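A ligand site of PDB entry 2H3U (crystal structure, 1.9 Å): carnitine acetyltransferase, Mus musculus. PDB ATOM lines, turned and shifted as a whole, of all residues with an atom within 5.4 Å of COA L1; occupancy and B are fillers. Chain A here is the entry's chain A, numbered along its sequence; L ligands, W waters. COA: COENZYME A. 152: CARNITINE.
NZ of Lys 397 is in salt-bridge range of O9A of COA L1, 3.0 Å away.
N of Asp 404 lies within hydrogen-bond range of O1A of COA L1 (2.7 Å).
NZ of Lys 393 is in salt-bridge range of O9A of COA L1, 2.8 Å away.
OG of Ser 402 lies within hydrogen-bond range of O2A of COA L1, 2.6 Å away.
The backbone NH (N) of Ser 430 sits at hydrogen-bond distance from an oxygen (O9P) of COA L1 (2.8 Å).
The side-chain hydroxyl (OG) of Ser 428 lies within hydrogen-bond range of an oxygen (O1B) of 152 L2 (2.7 Å).
NH1 of Arg 478 is in salt-bridge range of O4A of COA L1 (2.7 Å).
N of Gly 322 lies close to S1P of COA L1 (3.4 Å).
O of Gln 529 lies within hydrogen-bond range of N4P of COA L1.
O of Lys 400 is in hydrogen-bond range of N6A of COA L1 (3.1 Å).
The side-chain hydroxyl (OG1) of Thr 439 is in hydrogen-bond range of an oxygen (O1A) of 152 L2, 2.7 Å away.
O3 of 152 L2 sits at hydrogen-bond distance from NE2 of His 317 (2.8 Å).
Water W9 lies within hydrogen-bond range of O5P of COA L1 and OG of Ser 430.
Water W5 bridges an oxygen (OAP) of COA L1 (2.7 Å) and the guanidinium group (NH2) of Arg 478 (2.9 Å).
Water W3 lies within hydrogen-bond range of NE2 of Gln 529 and O1A of COA L1.
Water W16 lies within hydrogen-bond range of OG of Ser 528 (2.8 Å), S1P of COA L1 (2.9 Å) and O3 of 152 L2 (3.0 Å).
Water W1 lies within hydrogen-bond range of an oxygen (O4A) of COA L1 and the guanidinium group of Arg 478.
Water W15 bridges the side-chain amino group (NZ) of Lys 397 (3.0 Å) and an oxygen (O7A) of COA L1 (3.0 Å).
S1P of COA L1 lies close to O3 of 152 L2 (2.9 Å).
N of Pro 403 sits close to O1A of COA L1, 3.2 Å away.
Leu 137 touches COA L1 (CD1 to OAP, 3.3 Å).
His 317 touches COA L1.
Glu 321 touches COA L1.
Pro 323 touches COA L1.
N of Leu 401 touches N6A of COA L1, at 3.6 Å.
Ser 428 touches COA L1 (OG to C2P, 3.6 Å).
Ala 429 touches COA L1.
Ile 442 touches COA L1.
Thr 481 touches COA L1 (CG2 to CEP, 3.4 Å).
CG2 of Ile 485 touches OAP of COA L1, at 3.5 Å.
CB of Ser 528 touches C2P of COA L1 (3.9 Å).
Val 530 touches COA L1.
Hydrophobic or aromatic side chains within 4 Å of COA L1: Leu 137, His 317, Pro 323, Pro 403, Ile 442, Ile 485 and Val 530.
Within 4 Å of COA L1: Leu 137, His 317, Glu 321, Gly 322, Pro 323, Lys 393, Lys 397, Lys 400, Leu 401, Ser 402, Pro 403, Asp 404, Ser 428, Ala 429, Ser 430, Ile 442, Arg 478, Thr 481, Ile 485, Ser 528, Gln 529 and Val 530.
Along chain A the residues within 4 Å of COA L1 span positions 137 to 530.
NZ of Lys 397 lies within salt-bridge range of OE1 of Glu 556 (3.1 Å).
The side-chain carboxylate (OD2) of Asp 404 lies close to the side-chain carboxylate (OE2) of Glu 427 (2.6 Å).
The backbone NH (N) of Ala 405 is in hydrogen-bond range of the side-chain hydroxyl (OG) of Ser 402, at 3.3 Å.
The backbone NH of Lys 393 is in hydrogen-bond range of the backbone carbonyl oxygen of Glu 556, at 3.2 Å.
The backbone carbonyl oxygen (O) of Ile 442 lies within hydrogen-bond range of the backbone NH (N) of Glu 427.
OD1 of Asp 404 lies within hydrogen-bond range of NE2 of Gln 529.
The backbone NH of Gly 322 lies within hydrogen-bond range of the side-chain hydroxyl of Tyr 315 (3.3 Å).
N of Leu 401 is in hydrogen-bond range of O of Pro 396 (2.8 Å).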
ATOM      1  N   LEU A 137      -2.598 -13.376   9.671  1.00  0.00           N
ATOM      2  CA  LEU A 137      -3.045 -14.614  10.288  1.00  0.00           C
ATOM      3  C   LEU A 137      -1.818 -15.462  10.601  1.00  0.00           C
ATOM      4  O   LEU A 137      -1.926 -16.629  10.964  1.00  0.00           O
ATOM      5  CB  LEU A 137      -3.982 -15.367   9.337  1.00  0.00           C
ATOM      6  CG  LEU A 137      -5.155 -16.178   9.929  1.00  0.00           C
ATOM      7  CD1 LEU A 137      -4.644 -17.427  10.628  1.00  0.00           C
ATOM      8  CD2 LEU A 137      -5.936 -15.298  10.900  1.00  0.00           C
ATOM      9  N   TYR A 315     -26.366 -11.835  10.468  1.00  0.00           N
ATOM     10  CA  TYR A 315     -25.893 -11.349   9.177  1.00  0.00           C
ATOM     11  C   TYR A 315     -26.056 -12.388   8.079  1.00  0.00           C
ATOM     12  O   TYR A 315     -25.982 -13.588   8.339  1.00  0.00           O
ATOM     13  CB  TYR A 315     -24.429 -10.893   9.283  1.00  0.00           C
ATOM     14  CG  TYR A 315     -23.409 -12.007   9.306  1.00  0.00           C
ATOM     15  CD1 TYR A 315     -22.878 -12.512   8.116  1.00  0.00           C
ATOM     16  CD2 TYR A 315     -22.947 -12.535  10.501  1.00  0.00           C
ATOM     17  CE1 TYR A 315     -21.923 -13.515   8.125  1.00  0.00           C
ATOM     18  CE2 TYR A 315     -21.981 -13.553  10.523  1.00  0.00           C
ATOM     19  CZ  TYR A 315     -21.479 -14.028   9.321  1.00  0.00           C
ATOM     20  OH  TYR A 315     -20.512 -15.010   9.336  1.00  0.00           O
ATOM     21  N   HIS A 317     -24.888 -14.572   5.341  1.00  0.00           N
ATOM     22  CA  HIS A 317     -23.605 -15.218   5.057  1.00  0.00           C
ATOM     23  C   HIS A 317     -22.951 -15.085   3.693  1.00  0.00           C
ATOM     24  O   HIS A 317     -21.732 -15.226   3.585  1.00  0.00           O
ATOM     25  CB  HIS A 317     -23.706 -16.711   5.401  1.00  0.00           C
ATOM     26  CG  HIS A 317     -22.495 -17.258   6.081  1.00  0.00           C
ATOM     27  ND1 HIS A 317     -21.219 -16.833   5.780  1.00  0.00           N
ATOM     28  CD2 HIS A 317     -22.368 -18.206   7.042  1.00  0.00           C
ATOM     29  CE1 HIS A 317     -20.353 -17.505   6.529  1.00  0.00           C
ATOM     30  NE2 HIS A 317     -21.014 -18.340   7.301  1.00  0.00           N
ATOM     31  N   GLU A 321     -17.400 -13.916   6.265  1.00  0.00           N
ATOM     32  CA  GLU A 321     -17.253 -14.854   7.367  1.00  0.00           C
ATOM     33  C   GLU A 321     -17.315 -14.057   8.659  1.00  0.00           C
ATOM     34  O   GLU A 321     -17.433 -12.843   8.644  1.00  0.00           O
ATOM     35  CB  GLU A 321     -15.901 -15.579   7.305  1.00  0.00           C
ATOM     36  CG  GLU A 321     -15.947 -16.943   6.648  1.00  0.00           C
ATOM     37  CD  GLU A 321     -16.365 -16.847   5.209  1.00  0.00           C
ATOM     38  OE1 GLU A 321     -17.545 -17.073   4.912  1.00  0.00           O
ATOM     39  OE2 GLU A 321     -15.494 -16.530   4.365  1.00  0.00           O
ATOM     40  N   GLY A 322     -17.221 -14.764   9.783  1.00  0.00           N
ATOM     41  CA  GLY A 322     -17.284 -14.130  11.080  1.00  0.00           C
ATOM     42  C   GLY A 322     -16.207 -13.103  11.411  1.00  0.00           C
ATOM     43  O   GLY A 322     -16.543 -12.029  11.910  1.00  0.00           O
ATOM     44  N   PRO A 323     -14.929 -13.402  11.155  1.00  0.00           N
ATOM     45  CA  PRO A 323     -13.840 -12.461  11.455  1.00  0.00           C
ATOM     46  C   PRO A 323     -14.105 -11.006  11.070  1.00  0.00           C
ATOM     47  O   PRO A 323     -14.018 -10.108  11.922  1.00  0.00           O
ATOM     48  CB  PRO A 323     -12.654 -13.082  10.725  1.00  0.00           C
ATOM     49  CG  PRO A 323     -12.914 -14.547  10.923  1.00  0.00           C
ATOM     50  CD  PRO A 323     -14.399 -14.659  10.597  1.00  0.00           C
ATOM     51  N   LYS A 393      -7.979 -19.821  26.731  1.00  0.00           N
ATOM     52  CA  LYS A 393      -6.737 -20.084  26.024  1.00  0.00           C
ATOM     53  C   LYS A 393      -5.576 -20.191  26.997  1.00  0.00           C
ATOM     54  O   LYS A 393      -4.532 -20.778  26.688  1.00  0.00           O
ATOM     55  CB  LYS A 393      -6.453 -18.972  25.018  1.00  0.00           C
ATOM     56  CG  LYS A 393      -7.517 -18.814  23.940  1.00  0.00           C
ATOM     57  CD  LYS A 393      -7.124 -17.738  22.954  1.00  0.00           C
ATOM     58  CE  LYS A 393      -7.057 -16.383  23.631  1.00  0.00           C
ATOM     59  NZ  LYS A 393      -6.732 -15.295  22.671  1.00  0.00           N
ATOM     60  N   PRO A 396      -4.341 -24.150  27.812  1.00  0.00           N
ATOM     61  CA  PRO A 396      -3.665 -24.772  26.660  1.00  0.00           C
ATOM     62  C   PRO A 396      -2.313 -24.112  26.358  1.00  0.00           C
ATOM     63  O   PRO A 396      -1.322 -24.795  26.107  1.00  0.00           O
ATOM     64  CB  PRO A 396      -4.668 -24.568  25.530  1.00  0.00           C
ATOM     65  CG  PRO A 396      -5.983 -24.612  26.222  1.00  0.00           C
ATOM     66  CD  PRO A 396      -5.735 -23.815  27.487  1.00  0.00           C
ATOM     67  N   LYS A 397      -2.279 -22.789  26.399  1.00  0.00           N
ATOM     68  CA  LYS A 397      -1.033 -22.086  26.125  1.00  0.00           C
ATOM     69  C   LYS A 397       0.054 -22.437  27.149  1.00  0.00           C
ATOM     70  O   LYS A 397       1.211 -22.641  26.775  1.00  0.00           O
ATOM     71  CB  LYS A 397      -1.263 -20.574  26.072  1.00  0.00           C
ATOM     72  CG  LYS A 397      -1.950 -20.142  24.777  1.00  0.00           C
ATOM     73  CD  LYS A 397      -1.883 -18.648  24.520  1.00  0.00           C
ATOM     74  CE  LYS A 397      -2.730 -17.849  25.480  1.00  0.00           C
ATOM     75  NZ  LYS A 397      -2.769 -16.416  25.045  1.00  0.00           N
ATOM     76  N   LYS A 400       1.740 -25.373  26.236  1.00  0.00           N
ATOM     77  CA  LYS A 400       2.425 -25.299  24.940  1.00  0.00           C
ATOM     78  C   LYS A 400       1.566 -26.007  23.906  1.00  0.00           C
ATOM     79  O   LYS A 400       2.063 -26.726  23.041  1.00  0.00           O
ATOM     80  CB  LYS A 400       3.797 -25.984  24.990  1.00  0.00           C
ATOM     81  CG  LYS A 400       4.797 -25.342  25.944  1.00  0.00           C
ATOM     82  CD  LYS A 400       4.952 -23.861  25.660  1.00  0.00           C
ATOM     83  CE  LYS A 400       5.858 -23.192  26.683  1.00  0.00           C
ATOM     84  NZ  LYS A 400       5.887 -21.710  26.486  1.00  0.00           N
ATOM     85  N   LEU A 401       0.259 -25.810  23.999  1.00  0.00           N
ATOM     86  CA  LEU A 401      -0.668 -26.436  23.063  1.00  0.00           C
ATOM     87  C   LEU A 401      -1.578 -25.380  22.464  1.00  0.00           C
ATOM     88  O   LEU A 401      -1.919 -24.407  23.133  1.00  0.00           O
ATOM     89  CB  LEU A 401      -1.500 -27.506  23.764  1.00  0.00           C
ATOM     90  CG  LEU A 401      -0.797 -28.745  24.316  1.00  0.00           C
ATOM     91  CD1 LEU A 401      -1.800 -29.592  25.103  1.00  0.00           C
ATOM     92  CD2 LEU A 401      -0.204 -29.560  23.181  1.00  0.00           C
ATOM     93  N   SER A 402      -1.944 -25.580  21.209  1.00  0.00           N
ATOM     94  CA  SER A 402      -2.829 -24.652  20.508  1.00  0.00           C
ATOM     95  C   SER A 402      -4.219 -24.726  21.155  1.00  0.00           C
ATOM     96  O   SER A 402      -4.799 -25.806  21.259  1.00  0.00           O
ATOM     97  CB  SER A 402      -2.942 -25.052  19.035  1.00  0.00           C
ATOM     98  OG  SER A 402      -4.074 -24.456  18.436  1.00  0.00           O
ATOM     99  N   PRO A 403      -4.753 -23.581  21.611  1.00  0.00           N
ATOM    100  CA  PRO A 403      -6.089 -23.572  22.227  1.00  0.00           C
ATOM    101  C   PRO A 403      -7.151 -24.125  21.294  1.00  0.00           C
ATOM    102  O   PRO A 403      -7.949 -24.981  21.685  1.00  0.00           O
ATOM    103  CB  PRO A 403      -6.318 -22.092  22.528  1.00  0.00           C
ATOM    104  CG  PRO A 403      -4.939 -21.590  22.810  1.00  0.00           C
ATOM    105  CD  PRO A 403      -4.091 -22.282  21.760  1.00  0.00           C
ATOM    106  N   ASP A 404      -7.170 -23.655  20.041  1.00  0.00           N
ATOM    107  CA  ASP A 404      -8.158 -24.135  19.097  1.00  0.00           C
ATOM    108  C   ASP A 404      -8.083 -25.641  18.912  1.00  0.00           C
ATOM    109  O   ASP A 404      -9.115 -26.320  18.910  1.00  0.00           O
ATOM    110  CB  ASP A 404      -8.009 -23.470  17.731  1.00  0.00           C
ATOM    111  CG  ASP A 404      -9.184 -23.767  16.816  1.00  0.00           C
ATOM    112  OD1 ASP A 404     -10.317 -23.337  17.164  1.00  0.00           O
ATOM    113  OD2 ASP A 404      -8.995 -24.427  15.780  1.00  0.00           O
ATOM    114  N   ALA A 405      -6.874 -26.170  18.763  1.00  0.00           N
ATOM    115  CA  ALA A 405      -6.724 -27.611  18.588  1.00  0.00           C
ATOM    116  C   ALA A 405      -7.134 -28.334  19.864  1.00  0.00           C
ATOM    117  O   ALA A 405      -7.704 -29.421  19.819  1.00  0.00           O
ATOM    118  CB  ALA A 405      -5.276 -27.963  18.207  1.00  0.00           C
ATOM    119  N   GLU A 427     -14.421 -27.797  10.344  1.00  0.00           N
ATOM    120  CA  GLU A 427     -14.040 -26.606  11.083  1.00  0.00           C
ATOM    121  C   GLU A 427     -13.592 -25.577  10.065  1.00  0.00           C
ATOM    122  O   GLU A 427     -12.742 -25.846   9.220  1.00  0.00           O
ATOM    123  CB  GLU A 427     -12.896 -26.826  12.084  1.00  0.00           C
ATOM    124  CG  GLU A 427     -12.702 -25.552  12.935  1.00  0.00           C
ATOM    125  CD  GLU A 427     -11.401 -25.490  13.725  1.00  0.00           C
ATOM    126  OE1 GLU A 427     -10.635 -26.472  13.739  1.00  0.00           O
ATOM    127  OE2 GLU A 427     -11.157 -24.436  14.351  1.00  0.00           O
ATOM    128  N   SER A 428     -14.189 -24.387  10.136  1.00  0.00           N
ATOM    129  CA  SER A 428     -13.861 -23.308   9.226  1.00  0.00           C
ATOM    130  C   SER A 428     -12.393 -22.908   9.288  1.00  0.00           C
ATOM    131  O   SER A 428     -11.848 -22.725  10.383  1.00  0.00           O
ATOM    132  CB  SER A 428     -14.700 -22.069   9.533  1.00  0.00           C
ATOM    133  OG  SER A 428     -16.090 -22.346   9.454  1.00  0.00           O
ATOM    134  N   ALA A 429     -11.777 -22.782   8.117  1.00  0.00           N
ATOM    135  CA  ALA A 429     -10.388 -22.360   8.014  1.00  0.00           C
ATOM    136  C   ALA A 429     -10.395 -21.151   7.078  1.00  0.00           C
ATOM    137  O   ALA A 429     -10.972 -21.211   5.994  1.00  0.00           O
ATOM    138  CB  ALA A 429      -9.517 -23.464   7.445  1.00  0.00           C
ATOM    139  N   SER A 430      -9.770 -20.058   7.502  1.00  0.00           N
ATOM    140  CA  SER A 430      -9.728 -18.854   6.704  1.00  0.00           C
ATOM    141  C   SER A 430      -8.654 -18.881   5.636  1.00  0.00           C
ATOM    142  O   SER A 430      -7.488 -19.150   5.926  1.00  0.00           O
ATOM    143  CB  SER A 430      -9.496 -17.640   7.595  1.00  0.00           C
ATOM    144  OG  SER A 430      -9.345 -16.464   6.811  1.00  0.00           O
ATOM    145  N   THR A 439     -12.912 -19.518   2.601  1.00  0.00           N
ATOM    146  CA  THR A 439     -12.575 -20.595   3.519  1.00  0.00           C
ATOM    147  C   THR A 439     -12.247 -21.950   2.902  1.00  0.00           C
ATOM    148  O   THR A 439     -12.471 -22.183   1.715  1.00  0.00           O
ATOM    149  CB  THR A 439     -13.735 -20.851   4.496  1.00  0.00           C
ATOM    150  OG1 THR A 439     -14.846 -21.403   3.764  1.00  0.00           O
ATOM    151  CG2 THR A 439     -14.185 -19.551   5.169  1.00  0.00           C
ATOM    152  N   ILE A 442     -11.071 -27.795   7.630  1.00  0.00           N
ATOM    153  CA  ILE A 442     -10.117 -28.467   8.494  1.00  0.00           C
ATOM    154  C   ILE A 442     -10.978 -29.625   9.004  1.00  0.00           C
ATOM    155  O   ILE A 442     -12.101 -29.424   9.447  1.00  0.00           O
ATOM    156  CB  ILE A 442      -9.698 -27.582   9.679  1.00  0.00           C
ATOM    157  CG1 ILE A 442      -8.809 -26.461   9.187  1.00  0.00           C
ATOM    158  CG2 ILE A 442      -8.995 -28.437  10.754  1.00  0.00           C
ATOM    159  CD1 ILE A 442      -8.566 -25.371  10.224  1.00  0.00           C
ATOM    160  N   GLN A 475      -1.279 -31.686  17.993  1.00  0.00           N
ATOM    161  CA  GLN A 475      -0.271 -31.305  17.013  1.00  0.00           C
ATOM    162  C   GLN A 475      -0.727 -31.640  15.606  1.00  0.00           C
ATOM    163  O   GLN A 475      -0.513 -30.864  14.669  1.00  0.00           O
ATOM    164  CB  GLN A 475       1.057 -31.990  17.322  1.00  0.00           C
ATOM    165  CG  GLN A 475       1.778 -31.417  18.533  1.00  0.00           C
ATOM    166  CD  GLN A 475       2.033 -29.923  18.392  1.00  0.00           C
ATOM    167  OE1 GLN A 475       2.592 -29.468  17.386  1.00  0.00           O
ATOM    168  NE2 GLN A 475       1.630 -29.148  19.401  1.00  0.00           N
ATOM    169  N   ARG A 478      -3.078 -28.975  14.600  1.00  0.00           N
ATOM    170  CA  ARG A 478      -2.395 -27.708  14.330  1.00  0.00           C
ATOM    171  C   ARG A 478      -1.756 -27.765  12.942  1.00  0.00           C
ATOM    172  O   ARG A 478      -1.734 -26.773  12.212  1.00  0.00           O
ATOM    173  CB  ARG A 478      -1.306 -27.478  15.391  1.00  0.00           C
ATOM    174  CG  ARG A 478      -0.434 -26.260  15.143  1.00  0.00           C
ATOM    175  CD  ARG A 478      -1.229 -24.973  15.299  1.00  0.00           C
ATOM    176  NE  ARG A 478      -1.425 -24.292  14.019  1.00  0.00           N
ATOM    177  CZ  ARG A 478      -2.121 -23.171  13.861  1.00  0.00           C
ATOM    178  NH1 ARG A 478      -2.686 -22.583  14.906  1.00  0.00           N
ATOM    179  NH2 ARG A 478      -2.241 -22.624  12.659  1.00  0.00           N
ATOM    180  N   THR A 481      -4.353 -27.425  10.306  1.00  0.00           N
ATOM    181  CA  THR A 481      -4.748 -26.029  10.318  1.00  0.00           C
ATOM    182  C   THR A 481      -3.747 -25.182   9.517  1.00  0.00           C
ATOM    183  O   THR A 481      -4.143 -24.351   8.705  1.00  0.00           O
ATOM    184  CB  THR A 481      -4.808 -25.481  11.755  1.00  0.00           C
ATOM    185  OG1 THR A 481      -5.775 -26.224  12.506  1.00  0.00           O
ATOM    186  CG2 THR A 481      -5.199 -24.008  11.747  1.00  0.00           C
ATOM    187  N   ILE A 485      -4.956 -23.001   6.029  1.00  0.00           N
ATOM    188  CA  ILE A 485      -4.872 -21.572   5.792  1.00  0.00           C
ATOM    189  C   ILE A 485      -3.878 -21.260   4.685  1.00  0.00           C
ATOM    190  O   ILE A 485      -3.843 -20.144   4.184  1.00  0.00           O
ATOM    191  CB  ILE A 485      -4.466 -20.814   7.075  1.00  0.00           C
ATOM    192  CG1 ILE A 485      -3.143 -21.353   7.606  1.00  0.00           C
ATOM    193  CG2 ILE A 485      -5.581 -20.926   8.115  1.00  0.00           C
ATOM    194  CD1 ILE A 485      -2.691 -20.662   8.878  1.00  0.00           C
ATOM    195  N   SER A 528     -16.835 -23.850  13.998  1.00  0.00           N
ATOM    196  CA  SER A 528     -15.985 -22.715  13.650  1.00  0.00           C
ATOM    197  C   SER A 528     -15.620 -21.954  14.908  1.00  0.00           C
ATOM    198  O   SER A 528     -16.331 -21.994  15.923  1.00  0.00           O
ATOM    199  CB  SER A 528     -16.695 -21.761  12.676  1.00  0.00           C
ATOM    200  OG  SER A 528     -17.695 -21.018  13.347  1.00  0.00           O
ATOM    201  N   GLN A 529     -14.512 -21.244  14.814  1.00  0.00           N
ATOM    202  CA  GLN A 529     -14.033 -20.418  15.909  1.00  0.00           C
ATOM    203  C   GLN A 529     -14.166 -18.985  15.416  1.00  0.00           C
ATOM    204  O   GLN A 529     -13.838 -18.683  14.267  1.00  0.00           O
ATOM    205  CB  GLN A 529     -12.568 -20.723  16.208  1.00  0.00           C
ATOM    206  CG  GLN A 529     -12.070 -20.049  17.449  1.00  0.00           C
ATOM    207  CD  GLN A 529     -10.554 -19.972  17.495  1.00  0.00           C
ATOM    208  OE1 GLN A 529      -9.968 -19.140  16.820  1.00  0.00           O
ATOM    209  NE2 GLN A 529      -9.933 -20.846  18.264  1.00  0.00           N
ATOM    210  N   VAL A 530     -14.673 -18.116  16.278  1.00  0.00           N
ATOM    211  CA  VAL A 530     -14.821 -16.720  15.920  1.00  0.00           C
ATOM    212  C   VAL A 530     -14.286 -15.863  17.062  1.00  0.00           C
ATOM    213  O   VAL A 530     -15.041 -15.345  17.876  1.00  0.00           O
ATOM    214  CB  VAL A 530     -16.299 -16.343  15.637  1.00  0.00           C
ATOM    215  CG1 VAL A 530     -16.388 -14.893  15.206  1.00  0.00           C
ATOM    216  CG2 VAL A 530     -16.884 -17.261  14.561  1.00  0.00           C
ATOM    217  N   MET A 538     -21.140 -16.459  18.727  1.00  0.00           N
ATOM    218  CA  MET A 538     -21.963 -16.643  17.544  1.00  0.00           C
ATOM    219  C   MET A 538     -22.583 -18.038  17.525  1.00  0.00           C
ATOM    220  O   MET A 538     -22.173 -18.912  18.279  1.00  0.00           O
ATOM    221  CB  MET A 538     -21.136 -16.423  16.269  1.00  0.00           C
ATOM    222  CG  MET A 538     -20.423 -15.069  16.217  1.00  0.00           C
ATOM    223  SD  MET A 538     -20.075 -14.429  14.540  1.00  0.00           S
ATOM    224  CE  MET A 538     -19.970 -15.920  13.567  1.00  0.00           C
ATOM    225  N   GLU A 556      -9.370 -15.360  27.005  1.00  0.00           N
ATOM    226  CA  GLU A 556      -8.202 -15.756  27.781  1.00  0.00           C
ATOM    227  C   GLU A 556      -8.528 -16.647  28.971  1.00  0.00           C
ATOM    228  O   GLU A 556      -7.894 -17.686  29.169  1.00  0.00           O
ATOM    229  CB  GLU A 556      -7.441 -14.510  28.263  1.00  0.00           C
ATOM    230  CG  GLU A 556      -6.120 -14.795  28.969  1.00  0.00           C
ATOM    231  CD  GLU A 556      -5.135 -15.584  28.107  1.00  0.00           C
ATOM    232  OE1 GLU A 556      -5.112 -15.394  26.868  1.00  0.00           O
ATOM    233  OE2 GLU A 556      -4.362 -16.396  28.668  1.00  0.00           O
HETATM  234  N1A COA L   1       1.908 -22.785  22.788  1.00  0.00           N
HETATM  235  C2A COA L   1       1.521 -21.623  23.335  1.00  0.00           C
HETATM  236  N3A COA L   1       0.662 -20.818  22.694  1.00  0.00           N
HETATM  237  C4A COA L   1       0.148 -21.172  21.495  1.00  0.00           C
HETATM  238  C5A COA L   1       0.519 -22.375  20.906  1.00  0.00           C
HETATM  239  C6A COA L   1       1.421 -23.190  21.594  1.00  0.00           C
HETATM  240  N6A COA L   1       1.809 -24.346  21.069  1.00  0.00           N
HETATM  241  N7A COA L   1      -0.116 -22.480  19.747  1.00  0.00           N
HETATM  242  C8A COA L   1      -0.874 -21.383  19.593  1.00  0.00           C
HETATM  243  N9A COA L   1      -0.708 -20.578  20.666  1.00  0.00           N
HETATM  244  C1B COA L   1      -1.364 -19.252  20.906  1.00  0.00           C
HETATM  245  C2B COA L   1      -1.423 -18.368  19.677  1.00  0.00           C
HETATM  246  O2B COA L   1      -0.184 -17.639  19.575  1.00  0.00           O
HETATM  247  C3B COA L   1      -2.540 -17.415  20.018  1.00  0.00           C
HETATM  248  O3B COA L   1      -2.061 -16.431  20.932  1.00  0.00           O
HETATM  249  P3B COA L   1      -2.983 -15.181  21.337  1.00  0.00           P
HETATM  250  O7A COA L   1      -1.962 -14.176  22.075  1.00  0.00           O
HETATM  251  O8A COA L   1      -3.492 -14.556  20.097  1.00  0.00           O
HETATM  252  O9A COA L   1      -3.955 -15.656  22.348  1.00  0.00           O
HETATM  253  C4B COA L   1      -3.561 -18.309  20.728  1.00  0.00           C
HETATM  254  O4B COA L   1      -2.775 -19.413  21.319  1.00  0.00           O
HETATM  255  C5B COA L   1      -4.581 -18.928  19.741  1.00  0.00           C
HETATM  256  O5B COA L   1      -3.938 -19.755  18.765  1.00  0.00           O
HETATM  257  P1A COA L   1      -4.708 -21.063  18.205  1.00  0.00           P
HETATM  258  O1A COA L   1      -5.587 -21.574  19.294  1.00  0.00           O
HETATM  259  O2A COA L   1      -3.727 -21.989  17.589  1.00  0.00           O
HETATM  260  O3A COA L   1      -5.694 -20.463  17.066  1.00  0.00           O
HETATM  261  P2A COA L   1      -5.163 -19.599  15.806  1.00  0.00           P
HETATM  262  O4A COA L   1      -3.948 -20.216  15.223  1.00  0.00           O
HETATM  263  O5A COA L   1      -5.099 -18.162  16.193  1.00  0.00           O
HETATM  264  O6A COA L   1      -6.358 -19.773  14.759  1.00  0.00           O
HETATM  265  CBP COA L   1      -7.814 -20.885  13.161  1.00  0.00           C
HETATM  266  CCP COA L   1      -6.628 -21.036  14.118  1.00  0.00           C
HETATM  267  CDP COA L   1      -9.073 -20.537  13.984  1.00  0.00           C
HETATM  268  CEP COA L   1      -8.044 -22.215  12.424  1.00  0.00           C
HETATM  269  CAP COA L   1      -7.488 -19.741  12.160  1.00  0.00           C
HETATM  270  OAP COA L   1      -6.347 -20.095  11.387  1.00  0.00           O
HETATM  271  C9P COA L   1      -8.673 -19.456  11.241  1.00  0.00           C
HETATM  272  O9P COA L   1      -8.802 -20.029  10.162  1.00  0.00           O
HETATM  273  N8P COA L   1      -9.533 -18.550  11.721  1.00  0.00           N
HETATM  274  C7P COA L   1     -10.726 -18.132  10.995  1.00  0.00           C
HETATM  275  C6P COA L   1     -11.885 -19.132  11.237  1.00  0.00           C
HETATM  276  C5P COA L   1     -13.163 -18.581  10.619  1.00  0.00           C
HETATM  277  O5P COA L   1     -13.198 -18.274   9.428  1.00  0.00           O
HETATM  278  N4P COA L   1     -14.185 -18.463  11.465  1.00  0.00           N
HETATM  279  C3P COA L   1     -15.518 -17.911  11.062  1.00  0.00           C
HETATM  280  C2P COA L   1     -16.228 -18.835  10.079  1.00  0.00           C
HETATM  281  S1P COA L   1     -17.813 -18.122   9.511  1.00  0.00           S
HETATM  282  C1  152 L   2     -17.467 -21.573   6.124  1.00  0.00           C
HETATM  283  O1A 152 L   2     -17.353 -21.509   4.871  1.00  0.00           O
HETATM  284  O1B 152 L   2     -16.783 -22.352   6.819  1.00  0.00           O
HETATM  285  C2  152 L   2     -18.464 -20.661   6.826  1.00  0.00           C
HETATM  286  C3  152 L   2     -19.056 -21.279   8.107  1.00  0.00           C
HETATM  287  O3  152 L   2     -19.700 -20.243   8.852  1.00  0.00           O
HETATM  288  C4  152 L   2     -20.089 -22.329   7.710  1.00  0.00           C
HETATM  289  N5  152 L   2     -20.505 -23.164   8.856  1.00  0.00           N
HETATM  290  C5A 152 L   2     -19.334 -23.800   9.473  1.00  0.00           C
HETATM  291  C5B 152 L   2     -21.198 -22.348   9.849  1.00  0.00           C
HETATM  292  C5C 152 L   2     -21.411 -24.201   8.373  1.00  0.00           C
HETATM  293  O   HOH W   1      -1.236 -19.810  16.347  1.00  0.00           O
HETATM  294  O   HOH W   2       1.173 -17.908  23.608  1.00  0.00           O
HETATM  295  O   HOH W   3      -8.033 -20.253  19.818  1.00  0.00           O
HETATM  296  O   HOH W   4      -6.508 -16.445  14.780  1.00  0.00           O
HETATM  297  O   HOH W   5      -3.772 -20.166  12.293  1.00  0.00           O
HETATM  298  O   HOH W   6      -3.231 -12.852  24.331  1.00  0.00           O
HETATM  299  O   HOH W   7      -5.846 -14.769  19.031  1.00  0.00           O
HETATM  300  O   HOH W   8       5.020 -23.292  20.209  1.00  0.00           O
HETATM  301  O   HOH W   9     -12.631 -16.077   7.918  1.00  0.00           O
HETATM  302  O   HOH W  10       0.952 -15.595  21.123  1.00  0.00           O
HETATM  303  O   HOH W  11     -20.086 -17.037  10.941  1.00  0.00           O
HETATM  304  O   HOH W  12      -9.406 -17.018  13.913  1.00  0.00           O
HETATM  305  O   HOH W  13      -2.494 -13.846  17.678  1.00  0.00           O
HETATM  306  O   HOH W  14       0.683 -24.694  18.165  1.00  0.00           O
HETATM  307  O   HOH W  15      -0.165 -15.298  24.189  1.00  0.00           O
HETATM  308  O   HOH W  16     -19.171 -19.336  11.711  1.00  0.00           O
